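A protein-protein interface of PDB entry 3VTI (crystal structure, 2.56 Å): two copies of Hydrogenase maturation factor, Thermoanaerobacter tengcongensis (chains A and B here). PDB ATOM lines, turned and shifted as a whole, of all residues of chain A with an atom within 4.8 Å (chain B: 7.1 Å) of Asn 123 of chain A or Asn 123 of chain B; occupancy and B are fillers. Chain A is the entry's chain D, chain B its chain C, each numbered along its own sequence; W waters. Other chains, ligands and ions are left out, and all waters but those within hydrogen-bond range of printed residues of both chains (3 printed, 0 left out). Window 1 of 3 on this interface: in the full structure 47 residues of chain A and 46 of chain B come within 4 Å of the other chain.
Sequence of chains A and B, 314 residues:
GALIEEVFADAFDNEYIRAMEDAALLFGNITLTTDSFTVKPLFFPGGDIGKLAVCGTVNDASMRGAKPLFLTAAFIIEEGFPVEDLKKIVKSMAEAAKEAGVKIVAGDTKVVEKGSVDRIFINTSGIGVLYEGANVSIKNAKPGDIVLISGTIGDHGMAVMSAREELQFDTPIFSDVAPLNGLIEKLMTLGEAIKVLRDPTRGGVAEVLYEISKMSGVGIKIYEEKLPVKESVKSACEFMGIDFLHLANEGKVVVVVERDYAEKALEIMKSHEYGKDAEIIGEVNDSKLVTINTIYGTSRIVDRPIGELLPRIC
The backbone NH (N) of Thr 72 of chain A lies within hydrogen-bond range of the backbone carbonyl oxygen (O) of Ser 125 of chain A, at 2.8 Å. The side-chain hydroxyl (OG) of Ser 36 of chain B lies within hydrogen-bond range of the side-chain amide nitrogen (ND2) of Asn 123 of chain B (3.0 Å). The side-chain hydroxyl of Thr 34 of chain B sits at hydrogen-bond distance from the side-chain hydroxyl of Ser 125 of chain B (3.1 Å). The backbone carbonyl oxygen (O) of Thr 124 of chain A lies close to the side-chain hydroxyl (OG1) of Thr 34 of chain A. The backbone NH (N) of Ile 76 of chain B lies within hydrogen-bond range of the backbone carbonyl oxygen (O) of Phe 121 of chain B. The backbone NH (N) of Thr 72 of chain B sits at hydrogen-bond distance from the backbone carbonyl oxygen (O) of Ser 125 of chain B, 2.8 Å away.
OD1 of Asp 35 of chain A sits close to OD2 of Asp 108 of chain B, at 3.0 Å. OG of Ser 125 of chain A is in hydrogen-bond range of OG of Ser 125 of chain B (2.5 Å). The backbone NH of Ser 36 of chain A lies within hydrogen-bond range of the side-chain carboxylate of Asp 108 of chain B (3.3 Å).
Among the printed residues, pairs that only touch across the chains: Ala 74 of chain A with Asn 123 of chain B, Asn 123 of chain A with Ala 74 of chain B, Asn 123 of chain A with Asn 123 of chain B, Thr 34 of chain A with Thr 72 of chain B, Ser 36 of chain A with Ala 74 of chain B, Thr 72 of chain A with Thr 34 of chain B, Ala 74 of chain A with Ser 36 of chain B, Phe 121 of chain A with Ile 76 of chain B, Ser 36 of chain A with Ile 76 of chain B and Ser 125 of chain A with Thr 72 of chain B.
Ser 36 of chain A touches Ala 74 of chain B, and with the chains exchanged Ala 74 of chain A touches Ser 36 of chain B. Ala 74 of chain A touches Asn 123 of chain B, and with the chains exchanged Asn 123 of chain A touches Ala 74 of chain B. Asn 123 of chain B touches its own counterpart, Asn 123 of chain A. Ser 125 of chain A touches its own counterpart, Ser 125 of chain B. Positions printed for both chains: 34, 35, 36, 72, 73, 74, 121, 122, 123, 124 and 125. Of the 13 pairs that touch across the chains among the printed residues, 8 have their exchanged pair printed and touching as well.
Water W1 lies within hydrogen-bond range of OD1 of Asn 123 of chain A (2.6 Å), OG1 of Thr 72 of chain A (2.7 Å), OG1 of Thr 34 of chain B (3.0 Å) and OG of Ser 125 of chain A (3.2 Å). Water W2 lies within hydrogen-bond range of OG of Ser 36 of chain A, O of Phe 75 of chain B and OD2 of Asp 108 of chain B. Water W3 lies within hydrogen-bond range of the side-chain hydroxyl (OG1) of Thr 34 of chain A (2.9 Å), the side-chain amide oxygen (OD1) of Asn 123 of chain B (2.9 Å) and the side-chain hydroxyl (OG1) of Thr 72 of chain B (3.0 Å).
Of the 19 printed residues of chain B, 8 touch a printed residue of chain A. Hydrophobic or aromatic side chains of chain B within 4 Å of the printed part of chain A: Ala 74 and Ile 76. Of the 11 printed residues of chain A, 8 touch a printed residue of chain B. Printed residues of chain A that touch a printed residue of chain B: Thr 34, Asp 35, Ser 36, Thr 72, Ala 74, Phe 121, Asn 123 and Ser 125. Hydrophobic or aromatic side chains of chain A within 4 Å of the printed part of chain B: Ala 74 and Phe 121. Among the printed residues, no Asp or Glu carboxylate lies within 4 Å of a Lys or Arg side-chain nitrogen of the other chain.
Of the printed residues of chain B, Asn 123 of chain A touches Ala 74 (3.2 Å) and Asn 123 (3.5 Å). Of the printed residues of chain A, Ala 74 of chain B touches Ser 36 (3.6 Å) and Asn 123 (3.2 Å). Of the printed residues of chain B, Ser 36 of chain A touches Ala 74 (3.6 Å), Ile 76 (3.8 Å) and Asp 108 (3.3 Å). Printed residues of chain A within 4 Å of Thr 72 of chain B: Thr 34 (3.6 Å) and Ser 125 (3.9 Å). Of the printed residues of chain B, Ser 125 of chain A touches Thr 72 and Ser 125. The nearest printed residue of chain A that does not touch Ser 125 of chain B is Thr 72 of chain A (4.1 Å).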
ATOM      1  N   THR A  34      22.296  22.974  30.917  1.00  0.00           N
ATOM      2  CA  THR A  34      21.877  22.398  29.635  1.00  0.00           C
ATOM      3  C   THR A  34      20.882  21.273  29.886  1.00  0.00           C
ATOM      4  O   THR A  34      20.834  20.705  30.985  1.00  0.00           O
ATOM      5  CB  THR A  34      23.061  21.836  28.812  1.00  0.00           C
ATOM      6  OG1 THR A  34      22.609  21.458  27.502  1.00  0.00           O
ATOM      7  CG2 THR A  34      23.681  20.625  29.502  1.00  0.00           C
ATOM      8  N   ASP A  35      20.105  20.950  28.861  1.00  0.00           N
ATOM      9  CA  ASP A  35      19.110  19.912  28.972  1.00  0.00           C
ATOM     10  C   ASP A  35      18.660  19.483  27.585  1.00  0.00           C
ATOM     11  O   ASP A  35      18.562  20.310  26.678  1.00  0.00           O
ATOM     12  CB  ASP A  35      17.925  20.400  29.812  1.00  0.00           C
ATOM     13  CG  ASP A  35      17.115  19.263  30.402  1.00  0.00           C
ATOM     14  OD1 ASP A  35      17.503  18.085  30.216  1.00  0.00           O
ATOM     15  OD2 ASP A  35      16.088  19.551  31.056  1.00  0.00           O
ATOM     16  N   SER A  36      18.402  18.181  27.436  1.00  0.00           N
ATOM     17  CA  SER A  36      17.932  17.603  26.180  1.00  0.00           C
ATOM     18  C   SER A  36      16.484  17.193  26.313  1.00  0.00           C
ATOM     19  O   SER A  36      16.046  16.793  27.388  1.00  0.00           O
ATOM     20  CB  SER A  36      18.753  16.378  25.806  1.00  0.00           C
ATOM     21  OG  SER A  36      20.079  16.738  25.513  1.00  0.00           O
ATOM     22  N   THR A  72      20.647  28.848  24.096  1.00  0.00           N
ATOM     23  CA  THR A  72      21.098  28.262  22.856  1.00  0.00           C
ATOM     24  C   THR A  72      20.095  27.184  22.510  1.00  0.00           C
ATOM     25  O   THR A  72      19.407  26.677  23.390  1.00  0.00           O
ATOM     26  CB  THR A  72      22.485  27.625  22.979  1.00  0.00           C
ATOM     27  OG1 THR A  72      22.425  26.545  23.907  1.00  0.00           O
ATOM     28  CG2 THR A  72      23.537  28.636  23.427  1.00  0.00           C
ATOM     29  N   ALA A  73      20.010  26.844  21.228  1.00  0.00           N
ATOM     30  CA  ALA A  73      19.102  25.811  20.756  1.00  0.00           C
ATOM     31  C   ALA A  73      19.813  24.960  19.727  1.00  0.00           C
ATOM     32  O   ALA A  73      20.291  25.466  18.711  1.00  0.00           O
ATOM     33  CB  ALA A  73      17.850  26.428  20.158  1.00  0.00           C
ATOM     34  N   ALA A  74      19.886  23.665  20.003  1.00  0.00           N
ATOM     35  CA  ALA A  74      20.489  22.711  19.084  1.00  0.00           C
ATOM     36  C   ALA A  74      19.443  21.688  18.659  1.00  0.00           C
ATOM     37  O   ALA A  74      18.681  21.175  19.490  1.00  0.00           O
ATOM     38  CB  ALA A  74      21.673  22.029  19.732  1.00  0.00           C
ATOM     39  N   PHE A 121      15.232  15.657  18.091  1.00  0.00           N
ATOM     40  CA  PHE A 121      15.646  15.899  19.467  1.00  0.00           C
ATOM     41  C   PHE A 121      16.092  17.334  19.576  1.00  0.00           C
ATOM     42  O   PHE A 121      16.674  17.875  18.644  1.00  0.00           O
ATOM     43  CB  PHE A 121      16.780  14.963  19.891  1.00  0.00           C
ATOM     44  CG  PHE A 121      16.349  13.527  20.077  1.00  0.00           C
ATOM     45  CD1 PHE A 121      15.037  13.212  20.431  1.00  0.00           C
ATOM     46  CD2 PHE A 121      17.259  12.486  19.903  1.00  0.00           C
ATOM     47  CE1 PHE A 121      14.630  11.882  20.594  1.00  0.00           C
ATOM     48  CE2 PHE A 121      16.854  11.143  20.069  1.00  0.00           C
ATOM     49  CZ  PHE A 121      15.541  10.853  20.427  1.00  0.00           C
ATOM     50  N   ILE A 122      15.796  17.964  20.704  1.00  0.00           N
ATOM     51  CA  ILE A 122      16.254  19.326  20.934  1.00  0.00           C
ATOM     52  C   ILE A 122      17.066  19.422  22.219  1.00  0.00           C
ATOM     53  O   ILE A 122      16.668  18.883  23.255  1.00  0.00           O
ATOM     54  CB  ILE A 122      15.092  20.334  20.994  1.00  0.00           C
ATOM     55  CG1 ILE A 122      14.171  20.172  19.786  1.00  0.00           C
ATOM     56  CG2 ILE A 122      15.640  21.773  21.089  1.00  0.00           C
ATOM     57  CD1 ILE A 122      13.012  21.144  19.770  1.00  0.00           C
ATOM     58  N   ASN A 123      18.210  20.101  22.134  1.00  0.00           N
ATOM     59  CA  ASN A 123      18.945  20.496  23.322  1.00  0.00           C
ATOM     60  C   ASN A 123      18.943  21.994  23.460  1.00  0.00           C
ATOM     61  O   ASN A 123      19.123  22.713  22.481  1.00  0.00           O
ATOM     62  CB  ASN A 123      20.390  19.989  23.298  1.00  0.00           C
ATOM     63  CG  ASN A 123      21.210  20.513  24.481  1.00  0.00           C
ATOM     64  OD1 ASN A 123      21.586  21.689  24.517  1.00  0.00           O
ATOM     65  ND2 ASN A 123      21.470  19.649  25.458  1.00  0.00           N
ATOM     66  N   THR A 124      18.759  22.465  24.686  1.00  0.00           N
ATOM     67  CA  THR A 124      18.903  23.890  24.979  1.00  0.00           C
ATOM     68  C   THR A 124      19.834  24.097  26.165  1.00  0.00           C
ATOM     69  O   THR A 124      19.775  23.353  27.147  1.00  0.00           O
ATOM     70  CB  THR A 124      17.550  24.568  25.252  1.00  0.00           C
ATOM     71  OG1 THR A 124      16.801  23.776  26.176  1.00  0.00           O
ATOM     72  CG2 THR A 124      16.747  24.713  23.968  1.00  0.00           C
ATOM     73  N   SER A 125      20.708  25.093  26.053  1.00  0.00           N
ATOM     74  CA  SER A 125      21.527  25.535  27.167  1.00  0.00           C
ATOM     75  C   SER A 125      21.112  26.950  27.514  1.00  0.00           C
ATOM     76  O   SER A 125      20.584  27.660  26.660  1.00  0.00           O
ATOM     77  CB  SER A 125      23.005  25.524  26.803  1.00  0.00           C
ATOM     78  OG  SER A 125      23.412  24.244  26.381  1.00  0.00           O
ATOM     79  N   THR B  33      28.616  29.243  22.931  1.00  0.00           N
ATOM     80  CA  THR B  33      28.445  28.429  21.741  1.00  0.00           C
ATOM     81  C   THR B  33      27.748  27.115  22.073  1.00  0.00           C
ATOM     82  O   THR B  33      27.692  26.707  23.242  1.00  0.00           O
ATOM     83  CB  THR B  33      29.805  28.137  21.068  1.00  0.00           C
ATOM     84  OG1 THR B  33      29.608  27.371  19.871  1.00  0.00           O
ATOM     85  CG2 THR B  33      30.733  27.378  22.018  1.00  0.00           C
ATOM     86  N   THR B  34      27.205  26.459  21.053  1.00  0.00           N
ATOM     87  CA  THR B  34      26.701  25.107  21.210  1.00  0.00           C
ATOM     88  C   THR B  34      26.888  24.317  19.926  1.00  0.00           C
ATOM     89  O   THR B  34      26.810  24.878  18.847  1.00  0.00           O
ATOM     90  CB  THR B  34      25.219  25.067  21.659  1.00  0.00           C
ATOM     91  OG1 THR B  34      24.855  23.711  21.958  1.00  0.00           O
ATOM     92  CG2 THR B  34      24.289  25.619  20.578  1.00  0.00           C
ATOM     93  N   ASP B  35      27.148  23.022  20.055  1.00  0.00           N
ATOM     94  CA  ASP B  35      27.223  22.135  18.902  1.00  0.00           C
ATOM     95  C   ASP B  35      26.818  20.705  19.254  1.00  0.00           C
ATOM     96  O   ASP B  35      27.117  20.208  20.333  1.00  0.00           O
ATOM     97  CB  ASP B  35      28.628  22.143  18.302  1.00  0.00           C
ATOM     98  CG  ASP B  35      28.627  21.826  16.819  1.00  0.00           C
ATOM     99  OD1 ASP B  35      27.534  21.701  16.242  1.00  0.00           O
ATOM    100  OD2 ASP B  35      29.717  21.719  16.216  1.00  0.00           O
ATOM    101  N   SER B  36      26.126  20.057  18.324  1.00  0.00           N
ATOM    102  CA  SER B  36      25.807  18.632  18.439  1.00  0.00           C
ATOM    103  C   SER B  36      26.801  17.830  17.615  1.00  0.00           C
ATOM    104  O   SER B  36      27.386  18.352  16.661  1.00  0.00           O
ATOM    105  CB  SER B  36      24.380  18.338  17.975  1.00  0.00           C
ATOM    106  OG  SER B  36      23.432  18.880  18.875  1.00  0.00           O
ATOM    107  N   PHE B  37      26.991  16.571  17.995  1.00  0.00           N
ATOM    108  CA  PHE B  37      27.985  15.712  17.366  1.00  0.00           C
ATOM    109  C   PHE B  37      27.392  14.344  17.049  1.00  0.00           C
ATOM    110  O   PHE B  37      27.003  13.592  17.947  1.00  0.00           O
ATOM    111  CB  PHE B  37      29.215  15.613  18.263  1.00  0.00           C
ATOM    112  CG  PHE B  37      29.914  16.930  18.447  1.00  0.00           C
ATOM    113  CD1 PHE B  37      30.979  17.284  17.621  1.00  0.00           C
ATOM    114  CD2 PHE B  37      29.477  17.836  19.413  1.00  0.00           C
ATOM    115  CE1 PHE B  37      31.609  18.502  17.758  1.00  0.00           C
ATOM    116  CE2 PHE B  37      30.102  19.059  19.556  1.00  0.00           C
ATOM    117  CZ  PHE B  37      31.175  19.395  18.728  1.00  0.00           C
ATOM    118  N   ALA B  53      33.561  16.114  20.586  1.00  0.00           N
ATOM    119  CA  ALA B  53      32.547  16.901  21.271  1.00  0.00           C
ATOM    120  C   ALA B  53      33.163  18.022  22.122  1.00  0.00           C
ATOM    121  O   ALA B  53      32.594  19.109  22.237  1.00  0.00           O
ATOM    122  CB  ALA B  53      31.688  15.995  22.119  1.00  0.00           C
ATOM    123  N   THR B  57      33.753  22.425  20.553  1.00  0.00           N
ATOM    124  CA  THR B  57      33.159  23.491  21.338  1.00  0.00           C
ATOM    125  C   THR B  57      34.211  24.368  22.014  1.00  0.00           C
ATOM    126  O   THR B  57      34.006  25.573  22.175  1.00  0.00           O
ATOM    127  CB  THR B  57      32.185  22.922  22.352  1.00  0.00           C
ATOM    128  OG1 THR B  57      31.042  22.420  21.648  1.00  0.00           O
ATOM    129  CG2 THR B  57      31.749  23.984  23.347  1.00  0.00           C
ATOM    130  N   THR B  72      29.282  22.489  28.923  1.00  0.00           N
ATOM    131  CA  THR B  72      28.213  21.600  29.313  1.00  0.00           C
ATOM    132  C   THR B  72      28.281  20.382  28.415  1.00  0.00           C
ATOM    133  O   THR B  72      28.754  20.479  27.285  1.00  0.00           O
ATOM    134  CB  THR B  72      26.858  22.266  29.165  1.00  0.00           C
ATOM    135  OG1 THR B  72      26.753  22.807  27.851  1.00  0.00           O
ATOM    136  CG2 THR B  72      26.694  23.399  30.194  1.00  0.00           C
ATOM    137  N   ALA B  73      27.842  19.236  28.921  1.00  0.00           N
ATOM    138  CA  ALA B  73      27.853  18.007  28.135  1.00  0.00           C
ATOM    139  C   ALA B  73      26.516  17.285  28.231  1.00  0.00           C
ATOM    140  O   ALA B  73      26.112  16.851  29.306  1.00  0.00           O
ATOM    141  CB  ALA B  73      28.998  17.094  28.560  1.00  0.00           C
ATOM    142  N   ALA B  74      25.832  17.181  27.097  1.00  0.00           N
ATOM    143  CA  ALA B  74      24.573  16.473  27.034  1.00  0.00           C
ATOM    144  C   ALA B  74      24.713  15.206  26.189  1.00  0.00           C
ATOM    145  O   ALA B  74      25.233  15.249  25.072  1.00  0.00           O
ATOM    146  CB  ALA B  74      23.486  17.370  26.496  1.00  0.00           C
ATOM    147  N   PHE B  75      24.254  14.086  26.751  1.00  0.00           N
ATOM    148  CA  PHE B  75      24.361  12.780  26.130  1.00  0.00           C
ATOM    149  C   PHE B  75      22.974  12.215  25.872  1.00  0.00           C
ATOM    150  O   PHE B  75      22.135  12.170  26.776  1.00  0.00           O
ATOM    151  CB  PHE B  75      25.095  11.811  27.051  1.00  0.00           C
ATOM    152  CG  PHE B  75      26.487  12.229  27.409  1.00  0.00           C
ATOM    153  CD1 PHE B  75      26.725  13.011  28.542  1.00  0.00           C
ATOM    154  CD2 PHE B  75      27.564  11.810  26.642  1.00  0.00           C
ATOM    155  CE1 PHE B  75      28.009  13.389  28.892  1.00  0.00           C
ATOM    156  CE2 PHE B  75      28.854  12.182  26.977  1.00  0.00           C
ATOM    157  CZ  PHE B  75      29.078  12.977  28.114  1.00  0.00           C
ATOM    158  N   ILE B  76      22.737  11.776  24.640  1.00  0.00           N
ATOM    159  CA  ILE B  76      21.499  11.100  24.294  1.00  0.00           C
ATOM    160  C   ILE B  76      21.866   9.678  23.860  1.00  0.00           C
ATOM    161  O   ILE B  76      22.475   9.501  22.803  1.00  0.00           O
ATOM    162  CB  ILE B  76      20.718  11.869  23.192  1.00  0.00           C
ATOM    163  CG1 ILE B  76      20.389  13.294  23.679  1.00  0.00           C
ATOM    164  CG2 ILE B  76      19.466  11.108  22.794  1.00  0.00           C
ATOM    165  CD1 ILE B  76      19.912  14.260  22.611  1.00  0.00           C
ATOM    166  N   MET B  93      36.687  12.564  26.534  1.00  0.00           N
ATOM    167  CA  MET B  93      36.174  13.876  26.906  1.00  0.00           C
ATOM    168  C   MET B  93      36.934  14.450  28.093  1.00  0.00           C
ATOM    169  O   MET B  93      37.316  15.623  28.074  1.00  0.00           O
ATOM    170  CB  MET B  93      34.675  13.820  27.221  1.00  0.00           C
ATOM    171  CG  MET B  93      33.803  13.479  26.039  1.00  0.00           C
ATOM    172  SD  MET B  93      32.054  13.563  26.404  1.00  0.00           S
ATOM    173  CE  MET B  93      31.689  15.293  26.145  1.00  0.00           C
ATOM    174  N   ASP B 108      23.683  16.635  31.191  1.00  0.00           N
ATOM    175  CA  ASP B 108      22.460  15.867  31.163  1.00  0.00           C
ATOM    176  C   ASP B 108      22.748  14.538  30.497  1.00  0.00           C
ATOM    177  O   ASP B 108      23.622  14.451  29.636  1.00  0.00           O
ATOM    178  CB  ASP B 108      21.368  16.616  30.397  1.00  0.00           C
ATOM    179  CG  ASP B 108      20.002  15.968  30.548  1.00  0.00           C
ATOM    180  OD1 ASP B 108      19.606  15.639  31.697  1.00  0.00           O
ATOM    181  OD2 ASP B 108      19.325  15.781  29.512  1.00  0.00           O
ATOM    182  N   PHE B 121      24.402  10.260  20.567  1.00  0.00           N
ATOM    183  CA  PHE B 121      24.731  11.638  20.177  1.00  0.00           C
ATOM    184  C   PHE B 121      25.168  12.430  21.397  1.00  0.00           C
ATOM    185  O   PHE B 121      24.745  12.143  22.520  1.00  0.00           O
ATOM    186  CB  PHE B 121      23.550  12.359  19.512  1.00  0.00           C
ATOM    187  CG  PHE B 121      23.063  11.704  18.250  1.00  0.00           C
ATOM    188  CD1 PHE B 121      23.957  11.168  17.330  1.00  0.00           C
ATOM    189  CD2 PHE B 121      21.710  11.648  17.969  1.00  0.00           C
ATOM    190  CE1 PHE B 121      23.511  10.571  16.173  1.00  0.00           C
ATOM    191  CE2 PHE B 121      21.254  11.052  16.810  1.00  0.00           C
ATOM    192  CZ  PHE B 121      22.151  10.508  15.912  1.00  0.00           C
ATOM    193  N   ILE B 122      26.014  13.428  21.169  1.00  0.00           N
ATOM    194  CA  ILE B 122      26.468  14.305  22.229  1.00  0.00           C
ATOM    195  C   ILE B 122      26.347  15.772  21.814  1.00  0.00           C
ATOM    196  O   ILE B 122      26.749  16.157  20.708  1.00  0.00           O
ATOM    197  CB  ILE B 122      27.923  13.980  22.650  1.00  0.00           C
ATOM    198  CG1 ILE B 122      28.036  12.512  23.085  1.00  0.00           C
ATOM    199  CG2 ILE B 122      28.379  14.892  23.783  1.00  0.00           C
ATOM    200  CD1 ILE B 122      29.443  11.940  23.002  1.00  0.00           C
ATOM    201  N   ASN B 123      25.791  16.586  22.706  1.00  0.00           N
ATOM    202  CA  ASN B 123      25.831  18.025  22.545  1.00  0.00           C
ATOM    203  C   ASN B 123      26.709  18.665  23.605  1.00  0.00           C
ATOM    204  O   ASN B 123      26.648  18.293  24.777  1.00  0.00           O
ATOM    205  CB  ASN B 123      24.429  18.635  22.590  1.00  0.00           C
ATOM    206  CG  ASN B 123      24.455  20.148  22.428  1.00  0.00           C
ATOM    207  OD1 ASN B 123      24.800  20.878  23.359  1.00  0.00           O
ATOM    208  ND2 ASN B 123      24.126  20.624  21.232  1.00  0.00           N
ATOM    209  N   THR B 124      27.517  19.633  23.200  1.00  0.00           N
ATOM    210  CA  THR B 124      28.282  20.405  24.156  1.00  0.00           C
ATOM    211  C   THR B 124      28.040  21.887  23.945  1.00  0.00           C
ATOM    212  O   THR B 124      27.937  22.346  22.796  1.00  0.00           O
ATOM    213  CB  THR B 124      29.807  20.115  24.071  1.00  0.00           C
ATOM    214  OG1 THR B 124      30.247  20.178  22.711  1.00  0.00           O
ATOM    215  CG2 THR B 124      30.120  18.746  24.622  1.00  0.00           C
ATOM    216  N   SER B 125      27.926  22.627  25.047  1.00  0.00           N
ATOM    217  CA  SER B 125      27.954  24.091  24.988  1.00  0.00           C
ATOM    218  C   SER B 125      29.183  24.606  25.713  1.00  0.00           C
ATOM    219  O   SER B 125      29.748  23.911  26.566  1.00  0.00           O
ATOM    220  CB  SER B 125      26.691  24.704  25.590  1.00  0.00           C
ATOM    221  OG  SER B 125      25.534  24.158  24.980  1.00  0.00           O
HETATM  222  O   HOH W   1      22.242  23.921  23.367  1.00  0.00           O
HETATM  223  O   HOH W   2      21.270  14.963  27.381  1.00  0.00           O
HETATM  224  O   HOH W   3      25.117  20.839  26.276  1.00  0.00           O
